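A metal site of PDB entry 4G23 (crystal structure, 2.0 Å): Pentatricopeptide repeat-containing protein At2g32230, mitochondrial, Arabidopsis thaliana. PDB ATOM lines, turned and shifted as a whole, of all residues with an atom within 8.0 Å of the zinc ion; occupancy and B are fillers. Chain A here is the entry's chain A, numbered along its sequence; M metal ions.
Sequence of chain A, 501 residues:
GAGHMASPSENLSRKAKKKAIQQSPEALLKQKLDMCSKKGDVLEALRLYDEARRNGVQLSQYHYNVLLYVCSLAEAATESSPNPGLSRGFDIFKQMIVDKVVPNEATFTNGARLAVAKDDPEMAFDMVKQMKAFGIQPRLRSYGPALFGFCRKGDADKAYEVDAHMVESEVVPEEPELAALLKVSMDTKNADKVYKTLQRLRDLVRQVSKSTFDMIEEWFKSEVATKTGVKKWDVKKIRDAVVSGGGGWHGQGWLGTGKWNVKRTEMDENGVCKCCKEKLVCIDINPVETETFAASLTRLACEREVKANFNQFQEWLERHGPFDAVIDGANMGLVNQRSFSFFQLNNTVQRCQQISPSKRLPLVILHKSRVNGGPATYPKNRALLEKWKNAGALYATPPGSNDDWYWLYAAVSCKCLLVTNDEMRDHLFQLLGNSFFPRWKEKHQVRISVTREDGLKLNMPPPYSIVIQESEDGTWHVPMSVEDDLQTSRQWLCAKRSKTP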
ATOM      1  N   ASN A 261      -8.571  31.333   6.420  1.00  0.00           N
ATOM      2  CA  ASN A 261      -7.599  31.862   7.349  1.00  0.00           C
ATOM      3  C   ASN A 261      -6.224  31.421   6.875  1.00  0.00           C
ATOM      4  O   ASN A 261      -5.945  30.221   6.784  1.00  0.00           O
ATOM      5  CB  ASN A 261      -7.888  31.373   8.768  1.00  0.00           C
ATOM      6  CG  ASN A 261      -9.116  32.031   9.344  1.00  0.00           C
ATOM      7  OD1 ASN A 261     -10.042  31.361   9.805  1.00  0.00           O
ATOM      8  ND2 ASN A 261      -9.145  33.366   9.297  1.00  0.00           N
ATOM      9  N   LYS A 263      -2.168  31.867   7.359  1.00  0.00           N
ATOM     10  CA  LYS A 263      -1.102  32.311   8.285  1.00  0.00           C
ATOM     11  C   LYS A 263       0.271  31.801   7.873  1.00  0.00           C
ATOM     12  O   LYS A 263       0.405  30.683   7.386  1.00  0.00           O
ATOM     13  CB  LYS A 263      -1.367  31.837   9.711  1.00  0.00           C
ATOM     14  CG  LYS A 263      -2.722  32.182  10.312  1.00  0.00           C
ATOM     15  CD  LYS A 263      -2.816  33.654  10.694  1.00  0.00           C
ATOM     16  CE  LYS A 263      -4.258  34.049  11.029  1.00  0.00           C
ATOM     17  NZ  LYS A 263      -4.605  35.382  10.449  1.00  0.00           N
ATOM     18  N   THR A 265       3.554  30.256   9.222  1.00  0.00           N
ATOM     19  CA  THR A 265       3.684  29.426  10.406  1.00  0.00           C
ATOM     20  C   THR A 265       4.932  28.518  10.243  1.00  0.00           C
ATOM     21  O   THR A 265       5.770  28.778   9.386  1.00  0.00           O
ATOM     22  CB  THR A 265       2.382  28.646  10.665  1.00  0.00           C
ATOM     23  OG1 THR A 265       2.439  28.007  11.941  1.00  0.00           O
ATOM     24  CG2 THR A 265       2.115  27.583   9.613  1.00  0.00           C
ATOM     25  N   GLU A 266       5.054  27.522  11.101  1.00  0.00           N
ATOM     26  CA  GLU A 266       6.178  26.559  11.094  1.00  0.00           C
ATOM     27  C   GLU A 266       5.626  25.259  11.512  1.00  0.00           C
ATOM     28  O   GLU A 266       4.596  25.221  12.163  1.00  0.00           O
ATOM     29  CB  GLU A 266       7.231  26.929  12.130  1.00  0.00           C
ATOM     30  CG  GLU A 266       8.109  28.068  11.716  1.00  0.00           C
ATOM     31  CD  GLU A 266       9.022  28.568  12.847  1.00  0.00           C
ATOM     32  OE1 GLU A 266       8.939  28.068  13.998  1.00  0.00           O
ATOM     33  OE2 GLU A 266       9.842  29.443  12.559  1.00  0.00           O
ATOM     34  N   MET A 267       6.333  24.175  11.175  1.00  0.00           N
ATOM     35  CA  MET A 267       5.978  22.899  11.681  1.00  0.00           C
ATOM     36  C   MET A 267       6.935  22.645  12.817  1.00  0.00           C
ATOM     37  O   MET A 267       8.088  23.067  12.778  1.00  0.00           O
ATOM     38  CB  MET A 267       6.184  21.790  10.646  1.00  0.00           C
ATOM     39  CG  MET A 267       5.459  22.055   9.343  1.00  0.00           C
ATOM     40  SD  MET A 267       3.511  21.937   9.611  1.00  0.00           S
ATOM     41  CE  MET A 267       3.137  23.806   9.099  1.00  0.00           C
ATOM     42  N   VAL A 272       3.865  18.859  13.154  1.00  0.00           N
ATOM     43  CA  VAL A 272       2.598  19.426  13.642  1.00  0.00           C
ATOM     44  C   VAL A 272       2.562  20.919  13.324  1.00  0.00           C
ATOM     45  O   VAL A 272       3.489  21.650  13.655  1.00  0.00           O
ATOM     46  CB  VAL A 272       2.353  19.172  15.156  1.00  0.00           C
ATOM     47  CG1 VAL A 272       1.030  19.813  15.596  1.00  0.00           C
ATOM     48  CG2 VAL A 272       2.296  17.684  15.430  1.00  0.00           C
ATOM     49  N   CYS A 273       1.516  21.368  12.615  1.00  0.00           N
ATOM     50  CA  CYS A 273       1.359  22.775  12.250  1.00  0.00           C
ATOM     51  C   CYS A 273       1.139  23.573  13.532  1.00  0.00           C
ATOM     52  O   CYS A 273       0.284  23.222  14.311  1.00  0.00           O
ATOM     53  CB  CYS A 273       0.136  23.025  11.304  1.00  0.00           C
ATOM     54  SG  CYS A 273      -0.081  24.772  10.941  1.00  0.00           S
ATOM     55  N   LYS A 274       1.921  24.627  13.726  1.00  0.00           N
ATOM     56  CA  LYS A 274       1.824  25.391  14.975  1.00  0.00           C
ATOM     57  C   LYS A 274       0.588  26.279  14.969  1.00  0.00           C
ATOM     58  O   LYS A 274       0.076  26.646  16.009  1.00  0.00           O
ATOM     59  CB  LYS A 274       3.080  26.205  15.178  1.00  0.00           C
ATOM     60  CG  LYS A 274       4.252  25.319  15.626  1.00  0.00           C
ATOM     61  CD  LYS A 274       5.484  26.152  15.898  1.00  0.00           C
ATOM     62  CE  LYS A 274       6.735  25.314  16.129  1.00  0.00           C
ATOM     63  NZ  LYS A 274       7.920  26.186  15.907  1.00  0.00           N
ATOM     64  N   CYS A 275       0.074  26.563  13.773  1.00  0.00           N
ATOM     65  CA  CYS A 275      -1.156  27.327  13.622  1.00  0.00           C
ATOM     66  C   CYS A 275      -2.377  26.480  13.944  1.00  0.00           C
ATOM     67  O   CYS A 275      -3.130  26.810  14.842  1.00  0.00           O
ATOM     68  CB  CYS A 275      -1.252  27.874  12.206  1.00  0.00           C
ATOM     69  SG  CYS A 275      -2.748  28.842  11.935  1.00  0.00           S
ATOM     70  N   CYS A 276      -2.571  25.367  13.235  1.00  0.00           N
ATOM     71  CA  CYS A 276      -3.840  24.640  13.302  1.00  0.00           C
ATOM     72  C   CYS A 276      -3.728  23.294  13.984  1.00  0.00           C
ATOM     73  O   CYS A 276      -4.732  22.618  14.149  1.00  0.00           O
ATOM     74  CB  CYS A 276      -4.423  24.478  11.894  1.00  0.00           C
ATOM     75  SG  CYS A 276      -3.560  23.380  10.713  1.00  0.00           S
ATOM     76  N   LYS A 277      -2.513  22.885  14.331  1.00  0.00           N
ATOM     77  CA  LYS A 277      -2.247  21.604  14.989  1.00  0.00           C
ATOM     78  C   LYS A 277      -2.493  20.379  14.139  1.00  0.00           C
ATOM     79  O   LYS A 277      -2.561  19.288  14.652  1.00  0.00           O
ATOM     80  CB  LYS A 277      -3.007  21.445  16.327  1.00  0.00           C
ATOM     81  CG  LYS A 277      -2.941  22.636  17.255  1.00  0.00           C
ATOM     82  CD  LYS A 277      -1.558  23.203  17.440  1.00  0.00           C
ATOM     83  CE  LYS A 277      -1.617  24.427  18.350  1.00  0.00           C
ATOM     84  NZ  LYS A 277      -0.281  24.804  18.905  1.00  0.00           N
ATOM     85  N   GLU A 278      -2.612  20.543  12.829  1.00  0.00           N
ATOM     86  CA  GLU A 278      -2.695  19.375  11.997  1.00  0.00           C
ATOM     87  C   GLU A 278      -1.277  18.765  11.920  1.00  0.00           C
ATOM     88  O   GLU A 278      -0.283  19.461  11.924  1.00  0.00           O
ATOM     89  CB  GLU A 278      -3.226  19.709  10.615  1.00  0.00           C
ATOM     90  CG  GLU A 278      -3.109  18.561   9.615  1.00  0.00           C
ATOM     91  CD  GLU A 278      -4.309  18.433   8.696  1.00  0.00           C
ATOM     92  OE1 GLU A 278      -5.150  19.356   8.692  1.00  0.00           O
ATOM     93  OE2 GLU A 278      -4.411  17.403   7.997  1.00  0.00           O
ATOM     94  N   LYS A 279      -1.225  17.443  11.923  1.00  0.00           N
ATOM     95  CA  LYS A 279       0.011  16.723  11.766  1.00  0.00           C
ATOM     96  C   LYS A 279       0.194  16.320  10.296  1.00  0.00           C
ATOM     97  O   LYS A 279      -0.617  15.585   9.754  1.00  0.00           O
ATOM     98  CB  LYS A 279       0.004  15.514  12.685  1.00  0.00           C
ATOM     99  CG  LYS A 279       1.395  15.076  13.095  1.00  0.00           C
ATOM    100  CD  LYS A 279       1.896  13.962  12.225  1.00  0.00           C
ATOM    101  CE  LYS A 279       1.261  12.633  12.609  1.00  0.00           C
ATOM    102  NZ  LYS A 279       1.645  12.258  13.996  1.00  0.00           N
ATOM    103  N   LEU A 280       1.245  16.782   9.658  1.00  0.00           N
ATOM    104  CA  LEU A 280       1.488  16.402   8.259  1.00  0.00           C
ATOM    105  C   LEU A 280       1.801  14.920   8.075  1.00  0.00           C
ATOM    106  O   LEU A 280       2.147  14.233   9.017  1.00  0.00           O
ATOM    107  CB  LEU A 280       2.583  17.260   7.649  1.00  0.00           C
ATOM    108  CG  LEU A 280       2.250  18.750   7.653  1.00  0.00           C
ATOM    109  CD1 LEU A 280       3.347  19.522   6.952  1.00  0.00           C
ATOM    110  CD2 LEU A 280       0.879  19.072   7.063  1.00  0.00           C
ATOM    111  N   THR A 475      -7.792  21.479   3.777  1.00  0.00           N
ATOM    112  CA  THR A 475      -6.788  22.391   4.371  1.00  0.00           C
ATOM    113  C   THR A 475      -5.443  22.235   3.650  1.00  0.00           C
ATOM    114  O   THR A 475      -5.044  21.100   3.336  1.00  0.00           O
ATOM    115  CB  THR A 475      -6.615  22.092   5.886  1.00  0.00           C
ATOM    116  OG1 THR A 475      -7.869  22.289   6.536  1.00  0.00           O
ATOM    117  CG2 THR A 475      -5.600  22.990   6.532  1.00  0.00           C
ATOM    118  N   TRP A 476      -4.758  23.345   3.397  1.00  0.00           N
ATOM    119  CA  TRP A 476      -3.458  23.337   2.731  1.00  0.00           C
ATOM    120  C   TRP A 476      -2.311  23.735   3.623  1.00  0.00           C
ATOM    121  O   TRP A 476      -2.428  24.689   4.387  1.00  0.00           O
ATOM    122  CB  TRP A 476      -3.466  24.261   1.548  1.00  0.00           C
ATOM    123  CG  TRP A 476      -4.341  23.769   0.442  1.00  0.00           C
ATOM    124  CD1 TRP A 476      -5.726  23.915   0.315  1.00  0.00           C
ATOM    125  CD2 TRP A 476      -3.917  23.073  -0.756  1.00  0.00           C
ATOM    126  NE1 TRP A 476      -6.169  23.339  -0.846  1.00  0.00           N
ATOM    127  CE2 TRP A 476      -5.129  22.811  -1.535  1.00  0.00           C
ATOM    128  CE3 TRP A 476      -2.699  22.626  -1.236  1.00  0.00           C
ATOM    129  CZ2 TRP A 476      -5.093  22.132  -2.723  1.00  0.00           C
ATOM    130  CZ3 TRP A 476      -2.679  21.978  -2.461  1.00  0.00           C
ATOM    131  CH2 TRP A 476      -3.854  21.723  -3.176  1.00  0.00           C
ATOM    132  N   HIS A 477      -1.167  23.061   3.452  1.00  0.00           N
ATOM    133  CA  HIS A 477       0.115  23.460   4.031  1.00  0.00           C
ATOM    134  C   HIS A 477       1.156  23.545   2.959  1.00  0.00           C
ATOM    135  O   HIS A 477       1.403  22.589   2.223  1.00  0.00           O
ATOM    136  CB  HIS A 477       0.474  22.498   5.143  1.00  0.00           C
ATOM    137  CG  HIS A 477      -0.465  22.548   6.288  1.00  0.00           C
ATOM    138  ND1 HIS A 477      -1.507  21.741   6.385  1.00  0.00           N
ATOM    139  CD2 HIS A 477      -0.536  23.401   7.386  1.00  0.00           C
ATOM    140  CE1 HIS A 477      -2.196  22.049   7.484  1.00  0.00           C
ATOM    141  NE2 HIS A 477      -1.593  23.037   8.098  1.00  0.00           N
ATOM    142  N   VAL A 478       1.747  24.720   2.808  1.00  0.00           N
ATOM    143  CA  VAL A 478       2.681  24.998   1.733  1.00  0.00           C
ATOM    144  C   VAL A 478       4.067  25.391   2.318  1.00  0.00           C
ATOM    145  O   VAL A 478       4.174  26.425   2.994  1.00  0.00           O
ATOM    146  CB  VAL A 478       2.170  26.124   0.833  1.00  0.00           C
ATOM    147  CG1 VAL A 478       3.184  26.497  -0.245  1.00  0.00           C
ATOM    148  CG2 VAL A 478       0.799  25.733   0.223  1.00  0.00           C
ATOM    149  N   TRP A 492       6.195  28.089   6.474  1.00  0.00           N
ATOM    150  CA  TRP A 492       5.070  27.448   5.825  1.00  0.00           C
ATOM    151  C   TRP A 492       3.875  28.374   5.803  1.00  0.00           C
ATOM    152  O   TRP A 492       3.769  29.287   6.636  1.00  0.00           O
ATOM    153  CB  TRP A 492       4.641  26.262   6.601  1.00  0.00           C
ATOM    154  CG  TRP A 492       5.585  25.085   6.573  1.00  0.00           C
ATOM    155  CD1 TRP A 492       6.832  24.958   7.216  1.00  0.00           C
ATOM    156  CD2 TRP A 492       5.344  23.816   5.904  1.00  0.00           C
ATOM    157  NE1 TRP A 492       7.370  23.712   6.973  1.00  0.00           N
ATOM    158  CE2 TRP A 492       6.521  22.960   6.222  1.00  0.00           C
ATOM    159  CE3 TRP A 492       4.313  23.299   5.119  1.00  0.00           C
ATOM    160  CZ2 TRP A 492       6.619  21.692   5.729  1.00  0.00           C
ATOM    161  CZ3 TRP A 492       4.422  21.990   4.644  1.00  0.00           C
ATOM    162  CH2 TRP A 492       5.561  21.205   4.946  1.00  0.00           C
ATOM    163  N   LEU A 493       2.957  28.073   4.886  1.00  0.00           N
ATOM    164  CA  LEU A 493       1.641  28.697   4.819  1.00  0.00           C
ATOM    165  C   LEU A 493       0.638  27.692   5.303  1.00  0.00           C
ATOM    166  O   LEU A 493       0.651  26.522   4.897  1.00  0.00           O
ATOM    167  CB  LEU A 493       1.345  29.132   3.388  1.00  0.00           C
ATOM    168  CG  LEU A 493       0.406  30.319   3.207  1.00  0.00           C
ATOM    169  CD1 LEU A 493       1.006  31.588   3.781  1.00  0.00           C
ATOM    170  CD2 LEU A 493       0.083  30.502   1.716  1.00  0.00           C
ATOM    171  N   CYS A 494      -0.214  28.117   6.226  1.00  0.00           N
ATOM    172  CA  CYS A 494      -1.345  27.305   6.661  1.00  0.00           C
ATOM    173  C   CYS A 494      -2.609  28.014   6.107  1.00  0.00           C
ATOM    174  O   CYS A 494      -2.837  29.163   6.444  1.00  0.00           O
ATOM    175  CB  CYS A 494      -1.435  27.278   8.171  1.00  0.00           C
ATOM    176  SG  CYS A 494      -2.911  26.467   8.852  1.00  0.00           S
ATOM    177  N   ALA A 495      -3.383  27.327   5.255  1.00  0.00           N
ATOM    178  CA  ALA A 495      -4.638  27.874   4.678  1.00  0.00           C
ATOM    179  C   ALA A 495      -5.760  26.939   5.019  1.00  0.00           C
ATOM    180  O   ALA A 495      -5.835  25.823   4.516  1.00  0.00           O
ATOM    181  CB  ALA A 495      -4.509  28.018   3.150  1.00  0.00           C
ATOM    182  N   LYS A 496      -6.653  27.400   5.925  1.00  0.00           N
ATOM    183  CA  LYS A 496      -7.738  26.602   6.465  1.00  0.00           C
ATOM    184  C   LYS A 496      -9.053  27.415   6.415  1.00  0.00           C
ATOM    185  O   LYS A 496      -9.045  28.592   6.734  1.00  0.00           O
ATOM    186  CB  LYS A 496      -7.436  26.272   7.924  1.00  0.00           C
ATOM    187  CG  LYS A 496      -8.398  25.298   8.577  1.00  0.00           C
ATOM    188  CD  LYS A 496      -7.860  24.860   9.943  1.00  0.00           C
ATOM    189  CE  LYS A 496      -8.435  23.540  10.450  1.00  0.00           C
ATOM    190  NZ  LYS A 496      -8.662  22.501   9.385  1.00  0.00           N
HETATM  191 ZN    ZN M   1      -2.136  24.374   9.725  1.00  0.00          ZN
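The side-chain sulfur (SG) of Cys 276 lies close to the backbone NH (N) of Glu 278 (3.7 Å).
The backbone NH of Cys 494 is in hydrogen-bond range of the backbone carbonyl oxygen of Lys 263.
The side-chain sulfur (SG) of Cys 273 sits close to the backbone NH (N) of Cys 275 (3.4 Å).
The backbone NH (N) of Cys 273 lies within hydrogen-bond range of the backbone carbonyl oxygen (O) of Glu 278, at 2.7 Å.
The backbone NH (N) of Cys 273 lies close to the side-chain sulfur (SD) of Met 267, 3.7 Å away.
Of the 23 residues printed, 4 come within 4 Å of the zinc ion.
The side-chain sulfur (SG) of Cys 276 is bound to the zinc ion.
A ring nitrogen (NE2) of His 477 binds the zinc ion.
SG of Cys 494 is bound to the zinc ion, 2.4 Å away.
SG of Cys 273 is bound to the zinc ion, 2.4 Å away.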
